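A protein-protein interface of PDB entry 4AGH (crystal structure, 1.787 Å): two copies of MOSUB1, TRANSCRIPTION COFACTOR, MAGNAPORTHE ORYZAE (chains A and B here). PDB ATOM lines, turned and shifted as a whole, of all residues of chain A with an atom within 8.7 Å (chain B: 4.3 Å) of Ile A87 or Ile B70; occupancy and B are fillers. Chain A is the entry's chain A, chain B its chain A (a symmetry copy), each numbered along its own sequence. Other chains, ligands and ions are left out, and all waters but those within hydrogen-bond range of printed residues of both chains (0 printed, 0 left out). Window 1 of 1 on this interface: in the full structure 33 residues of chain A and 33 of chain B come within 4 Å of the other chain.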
ATOM      1  N   ILE A  51      11.275   0.733  18.656  1.00  0.00           N
ATOM      2  CA  ILE A  51      11.578   1.596  19.791  1.00  0.00           C
ATOM      3  C   ILE A  51      12.072   2.971  19.351  1.00  0.00           C
ATOM      4  O   ILE A  51      12.331   3.843  20.184  1.00  0.00           O
ATOM      5  CB  ILE A  51      12.557   0.918  20.790  1.00  0.00           C
ATOM      6  CG1 ILE A  51      13.911   0.644  20.140  1.00  0.00           C
ATOM      7  CG2 ILE A  51      11.921  -0.357  21.354  1.00  0.00           C
ATOM      8  CD1 ILE A  51      14.999   0.195  21.162  1.00  0.00           C
ATOM      9  N   ARG A  56      14.796  -1.461  16.603  1.00  0.00           N
ATOM     10  CA  ARG A  56      13.796  -2.493  16.836  1.00  0.00           C
ATOM     11  C   ARG A  56      14.220  -3.375  17.980  1.00  0.00           C
ATOM     12  O   ARG A  56      15.418  -3.560  18.221  1.00  0.00           O
ATOM     13  CB  ARG A  56      13.689  -3.389  15.599  1.00  0.00           C
ATOM     14  CG  ARG A  56      13.258  -2.668  14.331  1.00  0.00           C
ATOM     15  CD  ARG A  56      13.192  -3.647  13.157  1.00  0.00           C
ATOM     16  NE  ARG A  56      12.725  -2.981  11.941  1.00  0.00           N
ATOM     17  CZ  ARG A  56      12.370  -3.612  10.828  1.00  0.00           C
ATOM     18  NH1 ARG A  56      12.432  -4.934  10.760  1.00  0.00           N
ATOM     19  NH2 ARG A  56      11.955  -2.915   9.777  1.00  0.00           N
ATOM     20  N   VAL A  57      13.236  -3.947  18.670  1.00  0.00           N
ATOM     21  CA  VAL A  57      13.506  -5.112  19.506  1.00  0.00           C
ATOM     22  C   VAL A  57      12.683  -6.261  18.921  1.00  0.00           C
ATOM     23  O   VAL A  57      11.490  -6.117  18.689  1.00  0.00           O
ATOM     24  CB  VAL A  57      13.149  -4.882  20.979  1.00  0.00           C
ATOM     25  CG1 VAL A  57      13.480  -6.130  21.791  1.00  0.00           C
ATOM     26  CG2 VAL A  57      13.927  -3.696  21.516  1.00  0.00           C
ATOM     27  N   GLY A  58      13.328  -7.382  18.648  1.00  0.00           N
ATOM     28  CA  GLY A  58      12.626  -8.490  18.029  1.00  0.00           C
ATOM     29  C   GLY A  58      13.064  -9.784  18.661  1.00  0.00           C
ATOM     30  O   GLY A  58      13.996  -9.796  19.455  1.00  0.00           O
ATOM     31  N   SER A  60      14.214 -13.696  17.620  1.00  0.00           N
ATOM     32  CA  SER A  60      14.594 -14.640  16.576  1.00  0.00           C
ATOM     33  C   SER A  60      14.864 -15.994  17.205  1.00  0.00           C
ATOM     34  O   SER A  60      15.053 -16.102  18.418  1.00  0.00           O
ATOM     35  CB  SER A  60      15.851 -14.153  15.840  1.00  0.00           C
ATOM     36  OG  SER A  60      17.001 -14.207  16.684  1.00  0.00           O
ATOM     37  N   PHE A  67      16.324 -15.581  20.943  1.00  0.00           N
ATOM     38  CA  PHE A  67      17.167 -14.412  21.210  1.00  0.00           C
ATOM     39  C   PHE A  67      16.350 -13.144  21.157  1.00  0.00           C
ATOM     40  O   PHE A  67      15.439 -13.005  20.329  1.00  0.00           O
ATOM     41  CB  PHE A  67      18.306 -14.339  20.212  1.00  0.00           C
ATOM     42  CG  PHE A  67      19.215 -15.519  20.291  1.00  0.00           C
ATOM     43  CD1 PHE A  67      18.922 -16.677  19.591  1.00  0.00           C
ATOM     44  CD2 PHE A  67      20.313 -15.502  21.132  1.00  0.00           C
ATOM     45  CE1 PHE A  67      19.742 -17.787  19.694  1.00  0.00           C
ATOM     46  CE2 PHE A  67      21.137 -16.603  21.235  1.00  0.00           C
ATOM     47  CZ  PHE A  67      20.851 -17.748  20.517  1.00  0.00           C
ATOM     48  N   ILE A  68      16.669 -12.220  22.061  1.00  0.00           N
ATOM     49  CA  ILE A  68      16.011 -10.932  22.072  1.00  0.00           C
ATOM     50  C   ILE A  68      16.990  -9.950  21.447  1.00  0.00           C
ATOM     51  O   ILE A  68      18.024  -9.619  22.032  1.00  0.00           O
ATOM     52  CB  ILE A  68      15.633 -10.470  23.496  1.00  0.00           C
ATOM     53  CG1 ILE A  68      14.586 -11.407  24.135  1.00  0.00           C
ATOM     54  CG2 ILE A  68      15.084  -9.055  23.465  1.00  0.00           C
ATOM     55  CD1 ILE A  68      15.172 -12.698  24.713  1.00  0.00           C
ATOM     56  N   ASN A  69      16.664  -9.498  20.244  1.00  0.00           N
ATOM     57  CA  ASN A  69      17.580  -8.680  19.466  1.00  0.00           C
ATOM     58  C   ASN A  69      17.224  -7.211  19.536  1.00  0.00           C
ATOM     59  O   ASN A  69      16.127  -6.816  19.170  1.00  0.00           O
ATOM     60  CB  ASN A  69      17.564  -9.137  18.017  1.00  0.00           C
ATOM     61  CG  ASN A  69      17.920 -10.593  17.873  1.00  0.00           C
ATOM     62  OD1 ASN A  69      19.036 -11.004  18.195  1.00  0.00           O
ATOM     63  ND2 ASN A  69      16.979 -11.388  17.370  1.00  0.00           N
ATOM     64  N   ILE A  70      18.154  -6.403  20.027  1.00  0.00           N
ATOM     65  CA  ILE A  70      17.954  -4.970  20.073  1.00  0.00           C
ATOM     66  C   ILE A  70      18.916  -4.385  19.044  1.00  0.00           C
ATOM     67  O   ILE A  70      20.128  -4.519  19.190  1.00  0.00           O
ATOM     68  CB  ILE A  70      18.295  -4.450  21.472  1.00  0.00           C
ATOM     69  CG1 ILE A  70      17.529  -5.267  22.524  1.00  0.00           C
ATOM     70  CG2 ILE A  70      17.991  -2.959  21.570  1.00  0.00           C
ATOM     71  CD1 ILE A  70      17.908  -4.933  23.964  1.00  0.00           C
ATOM     72  N   ARG A  71      18.394  -3.751  17.996  1.00  0.00           N
ATOM     73  CA  ARG A  71      19.281  -3.438  16.879  1.00  0.00           C
ATOM     74  C   ARG A  71      18.795  -2.258  16.071  1.00  0.00           C
ATOM     75  O   ARG A  71      17.597  -2.079  15.897  1.00  0.00           O
ATOM     76  CB  ARG A  71      19.407  -4.662  15.965  1.00  0.00           C
ATOM     77  CG  ARG A  71      20.419  -4.479  14.839  1.00  0.00           C
ATOM     78  CD  ARG A  71      20.844  -5.794  14.228  1.00  0.00           C
ATOM     79  NE  ARG A  71      21.398  -6.732  15.208  1.00  0.00           N
ATOM     80  CZ  ARG A  71      22.652  -6.730  15.654  1.00  0.00           C
ATOM     81  NH1 ARG A  71      23.527  -5.803  15.258  1.00  0.00           N
ATOM     82  NH2 ARG A  71      23.027  -7.654  16.537  1.00  0.00           N
ATOM     83  N   GLU A  72      19.742  -1.462  15.582  1.00  0.00           N
ATOM     84  CA  GLU A  72      19.417  -0.365  14.694  1.00  0.00           C
ATOM     85  C   GLU A  72      19.464  -0.850  13.256  1.00  0.00           C
ATOM     86  O   GLU A  72      20.409  -1.531  12.847  1.00  0.00           O
ATOM     87  CB  GLU A  72      20.400   0.790  14.884  1.00  0.00           C
ATOM     88  CG  GLU A  72      20.142   1.955  13.929  1.00  0.00           C
ATOM     89  CD  GLU A  72      20.960   3.180  14.268  1.00  0.00           C
ATOM     90  OE1 GLU A  72      21.123   3.479  15.466  1.00  0.00           O
ATOM     91  OE2 GLU A  72      21.437   3.854  13.329  1.00  0.00           O
ATOM     92  N   GLY A  83      21.666  -3.411  10.919  1.00  0.00           N
ATOM     93  CA  GLY A  83      23.005  -2.857  10.928  1.00  0.00           C
ATOM     94  C   GLY A  83      23.840  -3.401  12.072  1.00  0.00           C
ATOM     95  O   GLY A  83      23.428  -4.306  12.799  1.00  0.00           O
ATOM     96  N   LYS A  84      25.021  -2.820  12.233  1.00  0.00           N
ATOM     97  CA  LYS A  84      26.015  -3.317  13.167  1.00  0.00           C
ATOM     98  C   LYS A  84      25.779  -2.858  14.607  1.00  0.00           C
ATOM     99  O   LYS A  84      26.344  -3.420  15.541  1.00  0.00           O
ATOM    100  CB  LYS A  84      27.408  -2.890  12.704  1.00  0.00           C
ATOM    101  CG  LYS A  84      28.410  -4.031  12.675  1.00  0.00           C
ATOM    102  CD  LYS A  84      27.940  -5.136  11.740  1.00  0.00           C
ATOM    103  CE  LYS A  84      28.958  -6.262  11.662  1.00  0.00           C
ATOM    104  NZ  LYS A  84      28.483  -7.403  10.828  1.00  0.00           N
ATOM    105  N   LYS A  85      24.950  -1.839  14.791  1.00  0.00           N
ATOM    106  CA  LYS A  85      24.683  -1.346  16.136  1.00  0.00           C
ATOM    107  C   LYS A  85      23.542  -2.157  16.733  1.00  0.00           C
ATOM    108  O   LYS A  85      22.388  -1.971  16.375  1.00  0.00           O
ATOM    109  CB  LYS A  85      24.327   0.142  16.109  1.00  0.00           C
ATOM    110  CG  LYS A  85      25.466   1.045  15.596  1.00  0.00           C
ATOM    111  CD  LYS A  85      25.029   2.499  15.447  1.00  0.00           C
ATOM    112  CE  LYS A  85      26.167   3.362  14.891  1.00  0.00           C
ATOM    113  NZ  LYS A  85      25.749   4.775  14.660  1.00  0.00           N
ATOM    114  N   GLY A  86      23.869  -3.067  17.635  1.00  0.00           N
ATOM    115  CA  GLY A  86      22.851  -3.919  18.230  1.00  0.00           C
ATOM    116  C   GLY A  86      23.452  -5.090  18.966  1.00  0.00           C
ATOM    117  O   GLY A  86      24.669  -5.305  18.946  1.00  0.00           O
ATOM    118  N   ILE A  87      22.584  -5.873  19.595  1.00  0.00           N
ATOM    119  CA  ILE A  87      23.032  -7.021  20.354  1.00  0.00           C
ATOM    120  C   ILE A  87      21.889  -8.025  20.430  1.00  0.00           C
ATOM    121  O   ILE A  87      20.716  -7.636  20.454  1.00  0.00           O
ATOM    122  CB  ILE A  87      23.527  -6.582  21.748  1.00  0.00           C
ATOM    123  CG1 ILE A  87      24.166  -7.759  22.503  1.00  0.00           C
ATOM    124  CG2 ILE A  87      22.394  -5.955  22.540  1.00  0.00           C
ATOM    125  CD1 ILE A  87      24.884  -7.309  23.789  1.00  0.00           C
ATOM    126  N   GLY A  88      22.236  -9.310  20.392  1.00  0.00           N
ATOM    127  CA  GLY A  88      21.254 -10.371  20.515  1.00  0.00           C
ATOM    128  C   GLY A  88      21.394 -11.021  21.877  1.00  0.00           C
ATOM    129  O   GLY A  88      22.365 -11.730  22.133  1.00  0.00           O
ATOM    130  N   LEU A  89      20.442 -10.752  22.766  1.00  0.00           N
ATOM    131  CA  LEU A  89      20.499 -11.295  24.115  1.00  0.00           C
ATOM    132  C   LEU A  89      19.915 -12.700  24.168  1.00  0.00           C
ATOM    133  O   LEU A  89      18.906 -12.984  23.531  1.00  0.00           O
ATOM    134  CB  LEU A  89      19.696 -10.406  25.077  1.00  0.00           C
ATOM    135  CG  LEU A  89      20.146  -8.952  25.164  1.00  0.00           C
ATOM    136  CD1 LEU A  89      19.239  -8.213  26.144  1.00  0.00           C
ATOM    137  CD2 LEU A  89      21.608  -8.872  25.586  1.00  0.00           C
ATOM    138  N   THR A  90      20.545 -13.573  24.947  1.00  0.00           N
ATOM    139  CA  THR A  90      19.922 -14.840  25.292  1.00  0.00           C
ATOM    140  C   THR A  90      18.768 -14.558  26.243  1.00  0.00           C
ATOM    141  O   THR A  90      18.651 -13.454  26.795  1.00  0.00           O
ATOM    142  CB  THR A  90      20.913 -15.773  26.017  1.00  0.00           C
ATOM    143  OG1 THR A  90      21.252 -15.202  27.283  1.00  0.00           O
ATOM    144  CG2 THR A  90      22.188 -15.960  25.192  1.00  0.00           C
ATOM    145  N   GLN A  93      20.052 -13.682  29.667  1.00  0.00           N
ATOM    146  CA  GLN A  93      20.579 -12.317  29.718  1.00  0.00           C
ATOM    147  C   GLN A  93      19.430 -11.327  29.762  1.00  0.00           C
ATOM    148  O   GLN A  93      19.471 -10.336  30.492  1.00  0.00           O
ATOM    149  CB  GLN A  93      21.478 -12.034  28.506  1.00  0.00           C
ATOM    150  CG  GLN A  93      22.816 -12.755  28.587  1.00  0.00           C
ATOM    151  CD  GLN A  93      23.471 -12.916  27.231  1.00  0.00           C
ATOM    152  OE1 GLN A  93      23.026 -12.333  26.245  1.00  0.00           O
ATOM    153  NE2 GLN A  93      24.538 -13.714  27.177  1.00  0.00           N
ATOM    154  N   TYR A  94      18.389 -11.613  28.989  1.00  0.00           N
ATOM    155  CA  TYR A  94      17.220 -10.742  28.962  1.00  0.00           C
ATOM    156  C   TYR A  94      16.519 -10.727  30.326  1.00  0.00           C
ATOM    157  O   TYR A  94      16.158  -9.653  30.826  1.00  0.00           O
ATOM    158  CB  TYR A  94      16.256 -11.165  27.855  1.00  0.00           C
ATOM    159  CG  TYR A  94      14.935 -10.433  27.865  1.00  0.00           C
ATOM    160  CD1 TYR A  94      14.841  -9.122  27.410  1.00  0.00           C
ATOM    161  CD2 TYR A  94      13.781 -11.058  28.310  1.00  0.00           C
ATOM    162  CE1 TYR A  94      13.637  -8.452  27.414  1.00  0.00           C
ATOM    163  CE2 TYR A  94      12.564 -10.396  28.312  1.00  0.00           C
ATOM    164  CZ  TYR A  94      12.497  -9.097  27.863  1.00  0.00           C
ATOM    165  OH  TYR A  94      11.291  -8.438  27.867  1.00  0.00           O
ATOM    166  N   PHE A  97      18.503  -8.704  32.689  1.00  0.00           N
ATOM    167  CA  PHE A  97      18.208  -7.311  32.382  1.00  0.00           C
ATOM    168  C   PHE A  97      16.889  -6.889  33.038  1.00  0.00           C
ATOM    169  O   PHE A  97      16.811  -5.842  33.679  1.00  0.00           O
ATOM    170  CB  PHE A  97      18.171  -7.103  30.869  1.00  0.00           C
ATOM    171  CG  PHE A  97      17.687  -5.749  30.450  1.00  0.00           C
ATOM    172  CD1 PHE A  97      18.403  -4.609  30.769  1.00  0.00           C
ATOM    173  CD2 PHE A  97      16.503  -5.615  29.751  1.00  0.00           C
ATOM    174  CE1 PHE A  97      17.962  -3.360  30.369  1.00  0.00           C
ATOM    175  CE2 PHE A  97      16.053  -4.370  29.373  1.00  0.00           C
ATOM    176  CZ  PHE A  97      16.791  -3.239  29.677  1.00  0.00           C
ATOM    177  N   ILE A 101      16.157  -3.708  35.815  1.00  0.00           N
ATOM    178  CA  ILE A 101      15.379  -2.552  35.375  1.00  0.00           C
ATOM    179  C   ILE A 101      14.910  -1.615  36.516  1.00  0.00           C
ATOM    180  O   ILE A 101      14.999  -0.400  36.389  1.00  0.00           O
ATOM    181  CB  ILE A 101      14.212  -2.979  34.459  1.00  0.00           C
ATOM    182  CG1 ILE A 101      14.743  -3.269  33.046  1.00  0.00           C
ATOM    183  CG2 ILE A 101      13.145  -1.908  34.407  1.00  0.00           C
ATOM    184  CD1 ILE A 101      13.685  -3.815  32.101  1.00  0.00           C
ATOM    185  N   ILE A 104      17.942   0.423  37.295  1.00  0.00           N
ATOM    186  CA  ILE A 104      18.255   1.283  36.157  1.00  0.00           C
ATOM    187  C   ILE A 104      17.285   2.452  36.133  1.00  0.00           C
ATOM    188  O   ILE A 104      17.689   3.607  35.967  1.00  0.00           O
ATOM    189  CB  ILE A 104      18.118   0.515  34.833  1.00  0.00           C
ATOM    190  CG1 ILE A 104      19.216  -0.543  34.737  1.00  0.00           C
ATOM    191  CG2 ILE A 104      18.179   1.482  33.644  1.00  0.00           C
ATOM    192  CD1 ILE A 104      18.928  -1.599  33.667  1.00  0.00           C
ATOM    193  N   ARG B  55      28.530  -9.397  29.618  1.00  0.00           N
ATOM    194  CA  ARG B  55      27.585  -8.388  29.144  1.00  0.00           C
ATOM    195  C   ARG B  55      27.079  -7.510  30.275  1.00  0.00           C
ATOM    196  O   ARG B  55      26.787  -7.990  31.370  1.00  0.00           O
ATOM    197  CB  ARG B  55      26.425  -9.050  28.403  1.00  0.00           C
ATOM    198  CG  ARG B  55      26.941  -9.685  27.108  1.00  0.00           C
ATOM    199  CD  ARG B  55      25.893 -10.457  26.338  1.00  0.00           C
ATOM    200  NE  ARG B  55      26.421 -10.749  25.006  1.00  0.00           N
ATOM    201  CZ  ARG B  55      25.672 -11.026  23.942  1.00  0.00           C
ATOM    202  NH1 ARG B  55      24.351 -11.115  24.056  1.00  0.00           N
ATOM    203  NH2 ARG B  55      26.260 -11.247  22.769  1.00  0.00           N
ATOM    204  N   ARG B  56      26.980  -6.223  29.980  1.00  0.00           N
ATOM    205  CA  ARG B  56      26.622  -5.222  30.974  1.00  0.00           C
ATOM    206  C   ARG B  56      25.505  -4.356  30.455  1.00  0.00           C
ATOM    207  O   ARG B  56      25.382  -4.147  29.244  1.00  0.00           O
ATOM    208  CB  ARG B  56      27.819  -4.301  31.228  1.00  0.00           C
ATOM    209  CG  ARG B  56      29.054  -5.004  31.769  1.00  0.00           C
ATOM    210  CD  ARG B  56      30.191  -4.000  31.977  1.00  0.00           C
ATOM    211  NE  ARG B  56      31.369  -4.650  32.551  1.00  0.00           N
ATOM    212  CZ  ARG B  56      32.423  -4.003  33.032  1.00  0.00           C
ATOM    213  NH1 ARG B  56      32.465  -2.679  33.008  1.00  0.00           N
ATOM    214  NH2 ARG B  56      33.444  -4.686  33.537  1.00  0.00           N
ATOM    215  N   VAL B  57      24.705  -3.824  31.377  1.00  0.00           N
ATOM    216  CA  VAL B  57      23.871  -2.673  31.049  1.00  0.00           C
ATOM    217  C   VAL B  57      24.340  -1.531  31.954  1.00  0.00           C
ATOM    218  O   VAL B  57      24.454  -1.701  33.161  1.00  0.00           O
ATOM    219  CB  VAL B  57      22.376  -2.945  31.249  1.00  0.00           C
ATOM    220  CG1 VAL B  57      21.570  -1.707  30.864  1.00  0.00           C
ATOM    221  CG2 VAL B  57      21.950  -4.123  30.393  1.00  0.00           C
ATOM    222  N   ILE B  68      21.473   4.453  27.805  1.00  0.00           N
ATOM    223  CA  ILE B  68      21.427   3.149  28.429  1.00  0.00           C
ATOM    224  C   ILE B  68      22.173   2.207  27.496  1.00  0.00           C
ATOM    225  O   ILE B  68      21.704   1.888  26.400  1.00  0.00           O
ATOM    226  CB  ILE B  68      19.985   2.646  28.649  1.00  0.00           C
ATOM    227  CG1 ILE B  68      19.219   3.541  29.645  1.00  0.00           C
ATOM    228  CG2 ILE B  68      19.995   1.218  29.165  1.00  0.00           C
ATOM    229  CD1 ILE B  68      18.671   4.833  29.033  1.00  0.00           C
ATOM    230  N   ASN B  69      23.348   1.774  27.933  1.00  0.00           N
ATOM    231  CA  ASN B  69      24.236   0.997  27.083  1.00  0.00           C
ATOM    232  C   ASN B  69      24.167  -0.482  27.397  1.00  0.00           C
ATOM    233  O   ASN B  69      24.429  -0.896  28.516  1.00  0.00           O
ATOM    234  CB  ASN B  69      25.663   1.486  27.257  1.00  0.00           C
ATOM    235  CG  ASN B  69      25.806   2.954  26.951  1.00  0.00           C
ATOM    236  OD1 ASN B  69      25.588   3.385  25.818  1.00  0.00           O
ATOM    237  ND2 ASN B  69      26.191   3.736  27.956  1.00  0.00           N
ATOM    238  N   ILE B  70      23.792  -1.277  26.404  1.00  0.00           N
ATOM    239  CA  ILE B  70      23.763  -2.715  26.564  1.00  0.00           C
ATOM    240  C   ILE B  70      24.898  -3.252  25.700  1.00  0.00           C
ATOM    241  O   ILE B  70      24.873  -3.091  24.483  1.00  0.00           O
ATOM    242  CB  ILE B  70      22.420  -3.258  26.072  1.00  0.00           C
ATOM    243  CG1 ILE B  70      21.276  -2.485  26.744  1.00  0.00           C
ATOM    244  CG2 ILE B  70      22.329  -4.758  26.330  1.00  0.00           C
ATOM    245  CD1 ILE B  70      19.889  -2.842  26.212  1.00  0.00           C
ATOM    246  N   ARG B  71      25.904  -3.876  26.311  1.00  0.00           N
ATOM    247  CA  ARG B  71      27.113  -4.141  25.537  1.00  0.00           C
ATOM    248  C   ARG B  71      27.896  -5.314  26.075  1.00  0.00           C
ATOM    249  O   ARG B  71      27.952  -5.519  27.281  1.00  0.00           O
ATOM    250  CB  ARG B  71      28.005  -2.894  25.533  1.00  0.00           C
ATOM    251  CG  ARG B  71      29.232  -3.026  24.637  1.00  0.00           C
ATOM    252  CD  ARG B  71      29.849  -1.686  24.307  1.00  0.00           C
ATOM    253  NE  ARG B  71      28.907  -0.757  23.677  1.00  0.00           N
ATOM    254  CZ  ARG B  71      28.591  -0.738  22.385  1.00  0.00           C
ATOM    255  NH1 ARG B  71      29.097  -1.633  21.534  1.00  0.00           N
ATOM    256  NH2 ARG B  71      27.727   0.175  21.942  1.00  0.00           N
ATOM    257  N   GLU B  72      28.499  -6.074  25.166  1.00  0.00           N
ATOM    258  CA  GLU B  72      29.377  -7.159  25.555  1.00  0.00           C
ATOM    259  C   GLU B  72      30.799  -6.641  25.667  1.00  0.00           C
ATOM    260  O   GLU B  72      31.285  -5.926  24.784  1.00  0.00           O
ATOM    261  CB  GLU B  72      29.317  -8.293  24.532  1.00  0.00           C
ATOM    262  CG  GLU B  72      30.270  -9.442  24.859  1.00  0.00           C
ATOM    263  CD  GLU B  72      30.046 -10.653  23.983  1.00  0.00           C
ATOM    264  OE1 GLU B  72      28.880 -10.975  23.692  1.00  0.00           O
ATOM    265  OE2 GLU B  72      31.046 -11.293  23.590  1.00  0.00           O
ATOM    266  N   LYS B  85      29.806  -5.549  20.076  1.00  0.00           N
ATOM    267  CA  LYS B  85      28.453  -6.078  20.193  1.00  0.00           C
ATOM    268  C   LYS B  85      27.723  -5.310  21.285  1.00  0.00           C
ATOM    269  O   LYS B  85      27.967  -5.517  22.466  1.00  0.00           O
ATOM    270  CB  LYS B  85      28.482  -7.574  20.516  1.00  0.00           C
ATOM    271  CG  LYS B  85      29.131  -8.436  19.415  1.00  0.00           C
ATOM    272  CD  LYS B  85      29.271  -9.897  19.832  1.00  0.00           C
ATOM    273  CE  LYS B  85      29.961 -10.718  18.738  1.00  0.00           C
ATOM    274  NZ  LYS B  85      30.184 -12.136  19.145  1.00  0.00           N
ATOM    275  N   GLY B  86      26.837  -4.413  20.888  1.00  0.00           N
ATOM    276  CA  GLY B  86      26.119  -3.600  21.859  1.00  0.00           C
ATOM    277  C   GLY B  86      25.420  -2.432  21.212  1.00  0.00           C
ATOM    278  O   GLY B  86      25.558  -2.186  20.010  1.00  0.00           O
ATOM    279  N   ILE B  87      24.686  -1.686  22.029  1.00  0.00           N
ATOM    280  CA  ILE B  87      23.948  -0.544  21.532  1.00  0.00           C
ATOM    281  C   ILE B  87      23.731   0.429  22.683  1.00  0.00           C
ATOM    282  O   ILE B  87      23.597   0.010  23.839  1.00  0.00           O
ATOM    283  CB  ILE B  87      22.623  -1.002  20.887  1.00  0.00           C
ATOM    284  CG1 ILE B  87      21.907   0.174  20.201  1.00  0.00           C
ATOM    285  CG2 ILE B  87      21.736  -1.675  21.919  1.00  0.00           C
ATOM    286  CD1 ILE B  87      20.713  -0.288  19.347  1.00  0.00           C
ATOM    287  N   LEU B  89      21.192   3.064  23.946  1.00  0.00           N
ATOM    288  CA  LEU B  89      19.843   3.578  23.764  1.00  0.00           C
ATOM    289  C   LEU B  89      19.695   4.966  24.371  1.00  0.00           C
ATOM    290  O   LEU B  89      20.220   5.239  25.447  1.00  0.00           O
ATOM    291  CB  LEU B  89      18.827   2.648  24.445  1.00  0.00           C
ATOM    292  CG  LEU B  89      18.823   1.204  23.955  1.00  0.00           C
ATOM    293  CD1 LEU B  89      17.774   0.420  24.740  1.00  0.00           C
ATOM    294  CD2 LEU B  89      18.553   1.151  22.456  1.00  0.00           C
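The backbone NH (N) of Gly B86 sits at hydrogen-bond distance from the backbone carbonyl oxygen (O) of Gly A86 (3.0 Å). NH1 of Arg B55 is in hydrogen-bond range of O of Gly A88, 2.8 Å away. The side-chain amide oxygen (OE1) of Gln A93 is in hydrogen-bond range of the guanidinium group (NH1) of Arg B55 (2.8 Å).
The backbone carbonyl oxygen (O) of Ile A68 sits at hydrogen-bond distance from the backbone NH (N) of Leu A89, at 2.8 Å. The backbone NH (N) of Glu A72 lies within hydrogen-bond range of the backbone carbonyl oxygen (O) of Lys A85, at 2.8 Å. The backbone NH (N) of Thr A90 sits at hydrogen-bond distance from the side-chain amide oxygen (OE1) of Gln A93 (3.1 Å). O of Ile B68 is in hydrogen-bond range of N of Leu B89 (2.8 Å). The backbone carbonyl oxygen (O) of Ile B70 is in hydrogen-bond range of the backbone NH (N) of Ile B87 (2.8 Å). The backbone NH of Glu B72 lies within hydrogen-bond range of the backbone carbonyl oxygen of Lys B85, 2.8 Å away.
CD1 of Ile A70 touches CD1 of Ile B70, at 3.7 Å. Ile A70 touches Ile B87. Lys A85 touches Gly B86 (C to O, 3.8 Å). Lys B85 touches Gly A86 (C to O, 3.8 Å). Gly A86 touches Ile B87. CG1 of Ile A87 touches NH1 of Arg B55, 3.7 Å away. Ile A87 touches Lys B85. CA of Gly B86 touches CB of Ile A87, 3.95 Å away. Arg B55 touches Leu A89. Ile A104 touches Val B57 (CD1 to CG1, 3.9 Å).
Ile A87 touches just these residues of chain B: Arg B55, Ile B70, Lys B85 and Gly B86. Ile B70 touches two residues of chain A. Of chain A, only Lys A85, Gly A86 and Ile A87 come within 4 Å of Gly B86. Printed residues of chain A within 4 Å of Leu B89: Ile A51. Of the printed residues of chain B, Leu A89 touches Arg B55 (3.9 Å). Printed residues of chain B within 4 Å of Gly A86: Lys B85 (3.8 Å), Gly B86 (3.0 Å) and Ile B87 (3.95 Å). Printed residues of chain A within 4 Å of Val B57: Phe A97 (3.6 Å) and Ile A104 (3.9 Å). Gly A58 touches none of the printed residues of chain B. Ile A101 touches none of the printed residues of chain B. The nearest residue of chain A that does not touch Ile B70 is Leu A89 (4.2 Å). The nearest printed residue of chain A that does not touch Ile B87 is Glu A72 (4.1 Å).
Hydrophobic or aromatic side chains of chain A within 4 Å of the printed part of chain B: Ile A51, Ile A70, Ile A87, Leu A89, Phe A97 and Ile A104. Printed residues of chain B that touch a printed residue of chain A: Arg B55, Val B57, Ile B70, Lys B85, Gly B86, Ile B87 and Leu B89. Hydrophobic or aromatic side chains of chain B that line the printed part of chain A: Val B57, Ile B70, Ile B87 and Leu B89. Among the printed residues, no Asp or Glu carboxylate lies within 4 Å of a Lys or Arg side-chain nitrogen of the other chain.
Ile A70 touches its own counterpart, Ile B70. Ile A70 touches Ile B87, and with the chains exchanged Ile A87 touches Ile B70. Gly B86 touches its own counterpart, Gly A86. Gly A86 touches Ile B87, and with the chains exchanged Ile A87 touches Gly B86. Positions printed for both chains: 56, 57, 68, 69, 70, 71, 72, 85, 86, 87 and 89. Of the 17 pairs that touch across the chains among the printed residues, 10 have their exchanged pair printed and touching as well.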
